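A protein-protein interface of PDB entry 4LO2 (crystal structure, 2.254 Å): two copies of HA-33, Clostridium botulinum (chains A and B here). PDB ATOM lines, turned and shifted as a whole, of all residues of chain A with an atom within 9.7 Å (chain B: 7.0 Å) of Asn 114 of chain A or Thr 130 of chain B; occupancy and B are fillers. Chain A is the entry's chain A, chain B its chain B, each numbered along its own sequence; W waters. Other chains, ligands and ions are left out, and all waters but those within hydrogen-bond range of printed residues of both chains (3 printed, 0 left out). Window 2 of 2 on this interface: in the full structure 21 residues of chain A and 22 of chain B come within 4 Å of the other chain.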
ATOM      1  N   TRP A  74      -2.240  -2.725   1.475  1.00  0.00           N
ATOM      2  CA  TRP A  74      -2.807  -1.419   1.749  1.00  0.00           C
ATOM      3  C   TRP A  74      -1.925  -0.345   1.117  1.00  0.00           C
ATOM      4  O   TRP A  74      -0.726  -0.261   1.413  1.00  0.00           O
ATOM      5  CB  TRP A  74      -2.913  -1.199   3.258  1.00  0.00           C
ATOM      6  CG  TRP A  74      -3.186   0.242   3.644  1.00  0.00           C
ATOM      7  CD1 TRP A  74      -3.945   1.153   2.964  1.00  0.00           C
ATOM      8  CD2 TRP A  74      -2.683   0.924   4.800  1.00  0.00           C
ATOM      9  NE1 TRP A  74      -3.957   2.358   3.631  1.00  0.00           N
ATOM     10  CE2 TRP A  74      -3.185   2.247   4.760  1.00  0.00           C
ATOM     11  CE3 TRP A  74      -1.868   0.541   5.873  1.00  0.00           C
ATOM     12  CZ2 TRP A  74      -2.892   3.193   5.751  1.00  0.00           C
ATOM     13  CZ3 TRP A  74      -1.580   1.490   6.868  1.00  0.00           C
ATOM     14  CH2 TRP A  74      -2.085   2.797   6.786  1.00  0.00           C
ATOM     15  N   TRP A  94      -1.944  -8.520   8.021  1.00  0.00           N
ATOM     16  CA  TRP A  94      -3.306  -8.265   8.480  1.00  0.00           C
ATOM     17  C   TRP A  94      -3.574  -9.096   9.719  1.00  0.00           C
ATOM     18  O   TRP A  94      -3.128 -10.238   9.825  1.00  0.00           O
ATOM     19  CB  TRP A  94      -4.305  -8.668   7.377  1.00  0.00           C
ATOM     20  CG  TRP A  94      -4.033  -7.936   6.091  1.00  0.00           C
ATOM     21  CD1 TRP A  94      -3.254  -8.362   5.061  1.00  0.00           C
ATOM     22  CD2 TRP A  94      -4.498  -6.625   5.734  1.00  0.00           C
ATOM     23  NE1 TRP A  94      -3.203  -7.402   4.080  1.00  0.00           N
ATOM     24  CE2 TRP A  94      -3.956  -6.324   4.470  1.00  0.00           C
ATOM     25  CE3 TRP A  94      -5.311  -5.673   6.371  1.00  0.00           C
ATOM     26  CZ2 TRP A  94      -4.209  -5.112   3.815  1.00  0.00           C
ATOM     27  CZ3 TRP A  94      -5.565  -4.467   5.724  1.00  0.00           C
ATOM     28  CH2 TRP A  94      -5.025  -4.202   4.448  1.00  0.00           C
ATOM     29  N   LEU A  95      -4.320  -8.523  10.648  1.00  0.00           N
ATOM     30  CA  LEU A  95      -4.736  -9.216  11.852  1.00  0.00           C
ATOM     31  C   LEU A  95      -6.120  -9.772  11.588  1.00  0.00           C
ATOM     32  O   LEU A  95      -7.008  -9.058  11.124  1.00  0.00           O
ATOM     33  CB  LEU A  95      -4.802  -8.242  13.029  1.00  0.00           C
ATOM     34  CG  LEU A  95      -3.562  -7.389  13.292  1.00  0.00           C
ATOM     35  CD1 LEU A  95      -3.847  -6.447  14.472  1.00  0.00           C
ATOM     36  CD2 LEU A  95      -2.330  -8.250  13.558  1.00  0.00           C
ATOM     37  N   LEU A  97      -9.237 -10.934  13.252  1.00  0.00           N
ATOM     38  CA  LEU A  97      -9.874 -10.879  14.548  1.00  0.00           C
ATOM     39  C   LEU A  97     -11.267 -11.463  14.421  1.00  0.00           C
ATOM     40  O   LEU A  97     -12.127 -10.902  13.753  1.00  0.00           O
ATOM     41  CB  LEU A  97      -9.940  -9.429  15.037  1.00  0.00           C
ATOM     42  CG  LEU A  97      -8.578  -8.752  15.008  1.00  0.00           C
ATOM     43  CD1 LEU A  97      -8.729  -7.248  15.193  1.00  0.00           C
ATOM     44  CD2 LEU A  97      -7.675  -9.366  16.080  1.00  0.00           C
ATOM     45  N   ILE A 106     -13.211  -9.303  11.642  1.00  0.00           N
ATOM     46  CA  ILE A 106     -12.694  -7.988  11.316  1.00  0.00           C
ATOM     47  C   ILE A 106     -11.251  -8.199  10.855  1.00  0.00           C
ATOM     48  O   ILE A 106     -10.505  -8.976  11.451  1.00  0.00           O
ATOM     49  CB  ILE A 106     -12.757  -7.063  12.539  1.00  0.00           C
ATOM     50  CG1 ILE A 106     -14.217  -6.808  12.899  1.00  0.00           C
ATOM     51  CG2 ILE A 106     -12.013  -5.740  12.259  1.00  0.00           C
ATOM     52  CD1 ILE A 106     -14.415  -5.953  14.152  1.00  0.00           C
ATOM     53  N   ILE A 107     -10.866  -7.540   9.775  1.00  0.00           N
ATOM     54  CA  ILE A 107      -9.526  -7.724   9.219  1.00  0.00           C
ATOM     55  C   ILE A 107      -8.777  -6.405   9.343  1.00  0.00           C
ATOM     56  O   ILE A 107      -9.045  -5.457   8.598  1.00  0.00           O
ATOM     57  CB  ILE A 107      -9.597  -8.156   7.724  1.00  0.00           C
ATOM     58  CG1 ILE A 107     -10.323  -9.500   7.600  1.00  0.00           C
ATOM     59  CG2 ILE A 107      -8.195  -8.239   7.114  1.00  0.00           C
ATOM     60  CD1 ILE A 107     -10.738  -9.870   6.155  1.00  0.00           C
ATOM     61  N   ALA A 108      -7.845  -6.330  10.287  1.00  0.00           N
ATOM     62  CA  ALA A 108      -7.221  -5.043  10.585  1.00  0.00           C
ATOM     63  C   ALA A 108      -5.842  -4.958   9.970  1.00  0.00           C
ATOM     64  O   ALA A 108      -5.142  -5.943   9.917  1.00  0.00           O
ATOM     65  CB  ALA A 108      -7.148  -4.819  12.121  1.00  0.00           C
ATOM     66  N   SER A 109      -5.442  -3.773   9.513  1.00  0.00           N
ATOM     67  CA  SER A 109      -4.080  -3.595   9.034  1.00  0.00           C
ATOM     68  C   SER A 109      -3.056  -3.830  10.143  1.00  0.00           C
ATOM     69  O   SER A 109      -3.173  -3.260  11.216  1.00  0.00           O
ATOM     70  CB  SER A 109      -3.894  -2.173   8.521  1.00  0.00           C
ATOM     71  OG  SER A 109      -2.557  -1.993   8.105  1.00  0.00           O
ATOM     72  N   TYR A 110      -2.042  -4.642   9.881  1.00  0.00           N
ATOM     73  CA  TYR A 110      -0.965  -4.813  10.855  1.00  0.00           C
ATOM     74  C   TYR A 110      -0.112  -3.541  10.957  1.00  0.00           C
ATOM     75  O   TYR A 110       0.372  -3.176  12.025  1.00  0.00           O
ATOM     76  CB  TYR A 110      -0.097  -6.018  10.484  1.00  0.00           C
ATOM     77  CG  TYR A 110       1.205  -6.098  11.273  1.00  0.00           C
ATOM     78  CD1 TYR A 110       1.222  -6.581  12.581  1.00  0.00           C
ATOM     79  CD2 TYR A 110       2.408  -5.687  10.712  1.00  0.00           C
ATOM     80  CE1 TYR A 110       2.401  -6.658  13.301  1.00  0.00           C
ATOM     81  CE2 TYR A 110       3.601  -5.755  11.433  1.00  0.00           C
ATOM     82  CZ  TYR A 110       3.582  -6.241  12.728  1.00  0.00           C
ATOM     83  OH  TYR A 110       4.746  -6.321  13.449  1.00  0.00           O
ATOM     84  N   LYS A 111       0.074  -2.879   9.823  1.00  0.00           N
ATOM     85  CA  LYS A 111       0.817  -1.631   9.755  1.00  0.00           C
ATOM     86  C   LYS A 111       0.163  -0.573  10.654  1.00  0.00           C
ATOM     87  O   LYS A 111       0.830   0.126  11.404  1.00  0.00           O
ATOM     88  CB  LYS A 111       0.849  -1.134   8.307  1.00  0.00           C
ATOM     89  CG  LYS A 111       2.115  -0.399   7.908  1.00  0.00           C
ATOM     90  CD  LYS A 111       2.098   1.028   8.335  1.00  0.00           C
ATOM     91  CE  LYS A 111       3.311   1.765   7.764  1.00  0.00           C
ATOM     92  NZ  LYS A 111       4.604   1.121   8.150  1.00  0.00           N
ATOM     93  N   ASN A 112      -1.150  -0.425  10.523  1.00  0.00           N
ATOM     94  CA  ASN A 112      -1.896   0.508  11.347  1.00  0.00           C
ATOM     95  C   ASN A 112      -3.253  -0.068  11.757  1.00  0.00           C
ATOM     96  O   ASN A 112      -4.246   0.096  11.049  1.00  0.00           O
ATOM     97  CB  ASN A 112      -2.101   1.845  10.653  1.00  0.00           C
ATOM     98  CG  ASN A 112      -2.646   2.907  11.618  1.00  0.00           C
ATOM     99  OD1 ASN A 112      -3.292   2.579  12.617  1.00  0.00           O
ATOM    100  ND2 ASN A 112      -2.372   4.167  11.333  1.00  0.00           N
ATOM    101  N   PRO A 113      -3.292  -0.726  12.917  1.00  0.00           N
ATOM    102  CA  PRO A 113      -4.492  -1.433  13.396  1.00  0.00           C
ATOM    103  C   PRO A 113      -5.650  -0.502  13.741  1.00  0.00           C
ATOM    104  O   PRO A 113      -6.740  -1.019  13.973  1.00  0.00           O
ATOM    105  CB  PRO A 113      -3.994  -2.181  14.641  1.00  0.00           C
ATOM    106  CG  PRO A 113      -2.497  -2.273  14.444  1.00  0.00           C
ATOM    107  CD  PRO A 113      -2.111  -1.001  13.751  1.00  0.00           C
ATOM    108  N   ASN A 114      -5.442   0.820  13.771  1.00  0.00           N
ATOM    109  CA  ASN A 114      -6.578   1.748  13.789  1.00  0.00           C
ATOM    110  C   ASN A 114      -7.491   1.495  12.583  1.00  0.00           C
ATOM    111  O   ASN A 114      -8.670   1.823  12.617  1.00  0.00           O
ATOM    112  CB  ASN A 114      -6.123   3.206  13.677  1.00  0.00           C
ATOM    113  CG  ASN A 114      -5.375   3.710  14.903  1.00  0.00           C
ATOM    114  OD1 ASN A 114      -4.908   4.846  14.915  1.00  0.00           O
ATOM    115  ND2 ASN A 114      -5.242   2.875  15.922  1.00  0.00           N
ATOM    116  N   LEU A 115      -6.926   0.965  11.498  1.00  0.00           N
ATOM    117  CA  LEU A 115      -7.662   0.823  10.238  1.00  0.00           C
ATOM    118  C   LEU A 115      -8.001  -0.638   9.908  1.00  0.00           C
ATOM    119  O   LEU A 115      -7.185  -1.535  10.108  1.00  0.00           O
ATOM    120  CB  LEU A 115      -6.856   1.438   9.090  1.00  0.00           C
ATOM    121  CG  LEU A 115      -6.636   2.948   9.234  1.00  0.00           C
ATOM    122  CD1 LEU A 115      -5.609   3.437   8.223  1.00  0.00           C
ATOM    123  CD2 LEU A 115      -7.969   3.704   9.063  1.00  0.00           C
ATOM    124  N   VAL A 116      -9.216  -0.865   9.410  1.00  0.00           N
ATOM    125  CA  VAL A 116      -9.688  -2.198   9.070  1.00  0.00           C
ATOM    126  C   VAL A 116     -10.337  -2.187   7.685  1.00  0.00           C
ATOM    127  O   VAL A 116     -10.759  -1.132   7.197  1.00  0.00           O
ATOM    128  CB  VAL A 116     -10.730  -2.722  10.114  1.00  0.00           C
ATOM    129  CG1 VAL A 116     -10.191  -2.620  11.545  1.00  0.00           C
ATOM    130  CG2 VAL A 116     -12.060  -1.964  10.012  1.00  0.00           C
ATOM    131  N   LEU A 117     -10.419  -3.360   7.050  1.00  0.00           N
ATOM    132  CA  LEU A 117     -11.057  -3.479   5.742  1.00  0.00           C
ATOM    133  C   LEU A 117     -12.534  -3.156   5.831  1.00  0.00           C
ATOM    134  O   LEU A 117     -13.223  -3.527   6.797  1.00  0.00           O
ATOM    135  CB  LEU A 117     -10.896  -4.893   5.173  1.00  0.00           C
ATOM    136  CG  LEU A 117      -9.496  -5.271   4.701  1.00  0.00           C
ATOM    137  CD1 LEU A 117      -9.509  -6.668   4.076  1.00  0.00           C
ATOM    138  CD2 LEU A 117      -9.012  -4.248   3.710  1.00  0.00           C
ATOM    139  N   LEU A 128      -9.900   1.016   3.378  1.00  0.00           N
ATOM    140  CA  LEU A 128      -9.625   0.956   4.803  1.00  0.00           C
ATOM    141  C   LEU A 128     -10.505   1.986   5.479  1.00  0.00           C
ATOM    142  O   LEU A 128     -10.804   3.030   4.905  1.00  0.00           O
ATOM    143  CB  LEU A 128      -8.149   1.227   5.104  1.00  0.00           C
ATOM    144  CG  LEU A 128      -7.243  -0.004   5.034  1.00  0.00           C
ATOM    145  CD1 LEU A 128      -5.911   0.307   5.638  1.00  0.00           C
ATOM    146  CD2 LEU A 128      -7.846  -1.151   5.780  1.00  0.00           C
ATOM    147  N   SER A 129     -10.929   1.680   6.696  1.00  0.00           N
ATOM    148  CA  SER A 129     -11.787   2.569   7.465  1.00  0.00           C
ATOM    149  C   SER A 129     -11.490   2.408   8.960  1.00  0.00           C
ATOM    150  O   SER A 129     -10.919   1.405   9.371  1.00  0.00           O
ATOM    151  CB  SER A 129     -13.250   2.215   7.181  1.00  0.00           C
ATOM    152  OG  SER A 129     -14.141   2.886   8.057  1.00  0.00           O
ATOM    153  N   THR A 130     -11.870   3.390   9.770  1.00  0.00           N
ATOM    154  CA  THR A 130     -11.882   3.190  11.213  1.00  0.00           C
ATOM    155  C   THR A 130     -13.084   2.304  11.571  1.00  0.00           C
ATOM    156  O   THR A 130     -13.933   2.016  10.720  1.00  0.00           O
ATOM    157  CB  THR A 130     -11.943   4.521  11.973  1.00  0.00           C
ATOM    158  OG1 THR A 130     -13.056   5.279  11.506  1.00  0.00           O
ATOM    159  CG2 THR A 130     -10.668   5.334  11.746  1.00  0.00           C
ATOM    160  N   LEU A 131     -13.144   1.848  12.812  1.00  0.00           N
ATOM    161  CA  LEU A 131     -14.146   0.856  13.204  1.00  0.00           C
ATOM    162  C   LEU A 131     -15.508   1.446  13.498  1.00  0.00           C
ATOM    163  O   LEU A 131     -15.635   2.620  13.848  1.00  0.00           O
ATOM    164  CB  LEU A 131     -13.686   0.067  14.425  1.00  0.00           C
ATOM    165  CG  LEU A 131     -12.496  -0.847  14.156  1.00  0.00           C
ATOM    166  CD1 LEU A 131     -11.193  -0.120  14.404  1.00  0.00           C
ATOM    167  CD2 LEU A 131     -12.592  -2.109  14.979  1.00  0.00           C
ATOM    168  N   ASN A 132     -16.523   0.604  13.363  1.00  0.00           N
ATOM    169  CA  ASN A 132     -17.882   0.963  13.725  1.00  0.00           C
ATOM    170  C   ASN A 132     -18.586  -0.359  14.007  1.00  0.00           C
ATOM    171  O   ASN A 132     -17.948  -1.411  13.995  1.00  0.00           O
ATOM    172  CB  ASN A 132     -18.547   1.688  12.564  1.00  0.00           C
ATOM    173  CG  ASN A 132     -18.436   0.898  11.266  1.00  0.00           C
ATOM    174  OD1 ASN A 132     -19.126  -0.097  11.078  1.00  0.00           O
ATOM    175  ND2 ASN A 132     -17.523   1.309  10.391  1.00  0.00           N
ATOM    176  N   ILE A 137     -17.653  -3.948   7.913  1.00  0.00           N
ATOM    177  CA  ILE A 137     -16.278  -4.268   8.315  1.00  0.00           C
ATOM    178  C   ILE A 137     -16.149  -5.718   8.781  1.00  0.00           C
ATOM    179  O   ILE A 137     -15.116  -6.123   9.329  1.00  0.00           O
ATOM    180  CB  ILE A 137     -15.740  -3.323   9.425  1.00  0.00           C
ATOM    181  CG1 ILE A 137     -16.608  -3.406  10.682  1.00  0.00           C
ATOM    182  CG2 ILE A 137     -15.667  -1.865   8.925  1.00  0.00           C
ATOM    183  CD1 ILE A 137     -15.894  -2.879  11.928  1.00  0.00           C
ATOM    184  N   PRO B 113     -16.317   1.311  19.186  1.00  0.00           N
ATOM    185  CA  PRO B 113     -15.470   0.179  18.798  1.00  0.00           C
ATOM    186  C   PRO B 113     -14.052   0.573  18.401  1.00  0.00           C
ATOM    187  O   PRO B 113     -13.220  -0.316  18.278  1.00  0.00           O
ATOM    188  CB  PRO B 113     -16.200  -0.424  17.593  1.00  0.00           C
ATOM    189  CG  PRO B 113     -17.555   0.123  17.631  1.00  0.00           C
ATOM    190  CD  PRO B 113     -17.488   1.453  18.316  1.00  0.00           C
ATOM    191  N   ASN B 114     -13.776   1.862  18.195  1.00  0.00           N
ATOM    192  CA  ASN B 114     -12.390   2.314  18.063  1.00  0.00           C
ATOM    193  C   ASN B 114     -11.576   2.192  19.353  1.00  0.00           C
ATOM    194  O   ASN B 114     -10.342   2.333  19.336  1.00  0.00           O
ATOM    195  CB  ASN B 114     -12.334   3.764  17.574  1.00  0.00           C
ATOM    196  CG  ASN B 114     -12.988   3.943  16.218  1.00  0.00           C
ATOM    197  OD1 ASN B 114     -14.060   4.534  16.107  1.00  0.00           O
ATOM    198  ND2 ASN B 114     -12.345   3.439  15.180  1.00  0.00           N
ATOM    199  N   LEU B 115     -12.259   1.955  20.467  1.00  0.00           N
ATOM    200  CA  LEU B 115     -11.603   1.907  21.766  1.00  0.00           C
ATOM    201  C   LEU B 115     -11.680   0.521  22.365  1.00  0.00           C
ATOM    202  O   LEU B 115     -12.733  -0.100  22.368  1.00  0.00           O
ATOM    203  CB  LEU B 115     -12.242   2.917  22.730  1.00  0.00           C
ATOM    204  CG  LEU B 115     -12.069   4.370  22.310  1.00  0.00           C
ATOM    205  CD1 LEU B 115     -12.810   5.268  23.300  1.00  0.00           C
ATOM    206  CD2 LEU B 115     -10.571   4.718  22.236  1.00  0.00           C
ATOM    207  N   VAL B 116     -10.551   0.046  22.882  1.00  0.00           N
ATOM    208  CA  VAL B 116     -10.447  -1.294  23.429  1.00  0.00           C
ATOM    209  C   VAL B 116      -9.776  -1.224  24.814  1.00  0.00           C
ATOM    210  O   VAL B 116      -9.041  -0.272  25.120  1.00  0.00           O
ATOM    211  CB  VAL B 116      -9.641  -2.232  22.463  1.00  0.00           C
ATOM    212  CG1 VAL B 116     -10.209  -2.159  21.038  1.00  0.00           C
ATOM    213  CG2 VAL B 116      -8.160  -1.837  22.434  1.00  0.00           C
ATOM    214  N   TYR B 118      -7.269  -1.717  27.780  1.00  0.00           N
ATOM    215  CA  TYR B 118      -5.825  -1.645  27.844  1.00  0.00           C
ATOM    216  C   TYR B 118      -5.432  -1.918  29.306  1.00  0.00           C
ATOM    217  O   TYR B 118      -5.925  -1.249  30.235  1.00  0.00           O
ATOM    218  CB  TYR B 118      -5.385  -0.228  27.427  1.00  0.00           C
ATOM    219  CG  TYR B 118      -3.889   0.017  27.433  1.00  0.00           C
ATOM    220  CD1 TYR B 118      -3.168   0.023  26.242  1.00  0.00           C
ATOM    221  CD2 TYR B 118      -3.200   0.248  28.622  1.00  0.00           C
ATOM    222  CE1 TYR B 118      -1.803   0.251  26.231  1.00  0.00           C
ATOM    223  CE2 TYR B 118      -1.826   0.473  28.618  1.00  0.00           C
ATOM    224  CZ  TYR B 118      -1.143   0.468  27.420  1.00  0.00           C
ATOM    225  OH  TYR B 118       0.207   0.693  27.395  1.00  0.00           O
ATOM    226  N   LEU B 128      -8.424   2.600  28.360  1.00  0.00           N
ATOM    227  CA  LEU B 128      -8.866   2.402  26.992  1.00  0.00           C
ATOM    228  C   LEU B 128      -7.809   2.891  26.017  1.00  0.00           C
ATOM    229  O   LEU B 128      -7.011   3.736  26.338  1.00  0.00           O
ATOM    230  CB  LEU B 128     -10.179   3.138  26.726  1.00  0.00           C
ATOM    231  CG  LEU B 128     -11.486   2.611  27.326  1.00  0.00           C
ATOM    232  CD1 LEU B 128     -12.595   3.521  26.884  1.00  0.00           C
ATOM    233  CD2 LEU B 128     -11.804   1.195  26.884  1.00  0.00           C
ATOM    234  N   SER B 129      -7.805   2.342  24.813  1.00  0.00           N
ATOM    235  CA  SER B 129      -6.843   2.757  23.819  1.00  0.00           C
ATOM    236  C   SER B 129      -7.434   2.465  22.462  1.00  0.00           C
ATOM    237  O   SER B 129      -8.285   1.596  22.322  1.00  0.00           O
ATOM    238  CB  SER B 129      -5.533   1.976  23.989  1.00  0.00           C
ATOM    239  OG  SER B 129      -4.638   2.209  22.915  1.00  0.00           O
ATOM    240  N   THR B 130      -6.985   3.193  21.456  1.00  0.00           N
ATOM    241  CA  THR B 130      -7.273   2.781  20.109  1.00  0.00           C
ATOM    242  C   THR B 130      -6.408   1.551  19.816  1.00  0.00           C
ATOM    243  O   THR B 130      -5.465   1.247  20.552  1.00  0.00           O
ATOM    244  CB  THR B 130      -6.986   3.914  19.133  1.00  0.00           C
ATOM    245  OG1 THR B 130      -5.662   4.416  19.367  1.00  0.00           O
ATOM    246  CG2 THR B 130      -8.008   5.042  19.350  1.00  0.00           C
ATOM    247  N   LEU B 131      -6.754   0.833  18.760  1.00  0.00           N
ATOM    248  CA  LEU B 131      -6.131  -0.441  18.444  1.00  0.00           C
ATOM    249  C   LEU B 131      -4.665  -0.270  18.049  1.00  0.00           C
ATOM    250  O   LEU B 131      -4.324   0.654  17.349  1.00  0.00           O
ATOM    251  CB  LEU B 131      -6.879  -1.080  17.286  1.00  0.00           C
ATOM    252  CG  LEU B 131      -7.946  -2.127  17.534  1.00  0.00           C
ATOM    253  CD1 LEU B 131      -8.561  -2.498  16.181  1.00  0.00           C
ATOM    254  CD2 LEU B 131      -7.298  -3.339  18.140  1.00  0.00           C
ATOM    255  N   ASN B 132      -3.814  -1.187  18.497  1.00  0.00           N
ATOM    256  CA  ASN B 132      -2.399  -1.207  18.140  1.00  0.00           C
ATOM    257  C   ASN B 132      -1.909  -2.650  18.256  1.00  0.00           C
ATOM    258  O   ASN B 132      -2.689  -3.544  18.568  1.00  0.00           O
ATOM    259  CB  ASN B 132      -1.609  -0.321  19.093  1.00  0.00           C
ATOM    260  CG  ASN B 132      -1.871  -0.670  20.552  1.00  0.00           C
ATOM    261  OD1 ASN B 132      -1.401  -1.686  21.045  1.00  0.00           O
ATOM    262  ND2 ASN B 132      -2.654   0.153  21.231  1.00  0.00           N
ATOM    263  N   ASN B 133      -0.617  -2.868  18.051  1.00  0.00           N
ATOM    264  CA  ASN B 133      -0.067  -4.209  18.161  1.00  0.00           C
ATOM    265  C   ASN B 133       0.544  -4.599  19.513  1.00  0.00           C
ATOM    266  O   ASN B 133       1.250  -5.599  19.599  1.00  0.00           O
ATOM    267  CB  ASN B 133       0.964  -4.427  17.061  1.00  0.00           C
ATOM    268  CG  ASN B 133       0.329  -4.461  15.697  1.00  0.00           C
ATOM    269  OD1 ASN B 133      -0.646  -5.186  15.485  1.00  0.00           O
ATOM    270  ND2 ASN B 133       0.839  -3.649  14.780  1.00  0.00           N
ATOM    271  N   ILE B 137      -3.264  -4.663  25.105  1.00  0.00           N
ATOM    272  CA  ILE B 137      -4.690  -4.758  24.746  1.00  0.00           C
ATOM    273  C   ILE B 137      -5.162  -6.199  24.489  1.00  0.00           C
ATOM    274  O   ILE B 137      -6.295  -6.429  24.055  1.00  0.00           O
ATOM    275  CB  ILE B 137      -5.062  -3.875  23.526  1.00  0.00           C
ATOM    276  CG1 ILE B 137      -4.384  -4.400  22.254  1.00  0.00           C
ATOM    277  CG2 ILE B 137      -4.674  -2.408  23.814  1.00  0.00           C
ATOM    278  CD1 ILE B 137      -4.981  -3.861  20.966  1.00  0.00           C
HETATM  279  O   HOH W   1     -14.869   5.052  13.411  1.00  0.00           O
HETATM  280  O   HOH W   2      -9.809   3.163  14.835  1.00  0.00           O
HETATM  281  O   HOH W   3      -5.212   6.614  17.289  1.00  0.00           O
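The side-chain amide nitrogen of Asn 133 of chain B is in hydrogen-bond range of the backbone carbonyl oxygen of Tyr 110 of chain A, at 2.8 Å.
The backbone carbonyl oxygen (O) of Leu 131 of chain B sits at hydrogen-bond distance from the side-chain amide nitrogen (ND2) of Asn 114 of chain A.
The backbone NH of Leu 131 of chain A lies close to the side-chain amide nitrogen of Asn 114 of chain B, at 3.0 Å.
The backbone carbonyl oxygen (O) of Ala 108 of chain A lies within hydrogen-bond range of the backbone NH (N) of Leu 95 of chain A, 2.8 Å away.
OD1 of Asn 112 of chain A sits at hydrogen-bond distance from N of Asn 114 of chain A, at 3.0 Å.
The side-chain hydroxyl of Ser 129 of chain B is in hydrogen-bond range of the side-chain amide nitrogen of Asn 132 of chain B (3.3 Å).
The side-chain amide nitrogen of Asn 132 of chain B is in hydrogen-bond range of the backbone carbonyl oxygen of Thr 130 of chain B (3.1 Å).
Asn 133 of chain B touches Leu 95 of chain A.
Pro 113 of chain A touches Leu 131 of chain B (O to CD1, 3.2 Å).
Pro 113 of chain A touches Asn 132 of chain B.
Pro 113 of chain A touches Asn 133 of chain B (CG to OD1, 3.6 Å).
Thr 130 of chain B touches Asn 114 of chain A (OG1 to ND2, 3.8 Å).
Thr 130 of chain A touches Asn 114 of chain B.
CD2 of Leu 131 of chain A touches O of Pro 113 of chain B, 3.8 Å away.
Leu 131 of chain A touches Leu 131 of chain B.
Asn 132 of chain A touches Pro 113 of chain B.
Of the printed residues of chain B, Leu 95 of chain A touches Asn 133.
Ser 129 of chain A touches none of the printed residues of chain B.
Printed residues of chain B within 4 Å of Thr 130 of chain A: Asn 114.
Of the printed residues of chain B, Leu 131 of chain A touches Pro 113, Asn 114 and Leu 131.
Printed residues of chain B within 4 Å of Asn 132 of chain A: Pro 113.
Of the printed residues of chain A, Asn 114 of chain B touches Thr 130 and Leu 131.
Printed residues of chain B that touch a printed residue of chain A: Pro 113, Asn 114, Thr 130, Leu 131, Asn 132 and Asn 133.
Of the 22 printed residues of chain A, 7 touch a printed residue of chain B.
Printed residues of chain A that touch a printed residue of chain B: Leu 95, Tyr 110, Pro 113, Asn 114, Thr 130, Leu 131 and Asn 132.
Hydrophobic or aromatic side chains of chain A that line the printed part of chain B: Leu 95, Tyr 110, Pro 113 and Leu 131.
Among the printed residues, no Asp or Glu carboxylate lies within 4 Å of a Lys or Arg side-chain nitrogen of the other chain.
Pro 113 of chain A touches Leu 131 of chain B, and with the chains exchanged Leu 131 of chain A touches Pro 113 of chain B.
Asn 114 of chain A touches Thr 130 of chain B, and with the chains exchanged Thr 130 of chain A touches Asn 114 of chain B.
Asn 114 of chain A touches Leu 131 of chain B, and with the chains exchanged Leu 131 of chain A touches Asn 114 of chain B.
Leu 131 of chain A touches its own counterpart, Leu 131 of chain B.
Positions printed for both chains: 113, 114, 115, 116, 128, 129, 130, 131, 132 and 137.
Of the 12 pairs that touch across the chains among the printed residues, 9 have their exchanged pair printed and touching as well.
Water W2 lies within hydrogen-bond range of the side-chain amide nitrogen (ND2) of Asn 114 of chain B (2.6 Å) and the backbone carbonyl oxygen (O) of Asn 114 of chain A (2.8 Å).
Water W1 lies within hydrogen-bond range of the backbone carbonyl oxygen of Leu 131 of chain A, the side-chain hydroxyl of Thr 130 of chain A and the side-chain amide oxygen of Asn 114 of chain B.
Water W3 lies within hydrogen-bond range of the side-chain amide oxygen of Asn 114 of chain A and the side-chain hydroxyl of Thr 130 of chain B.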
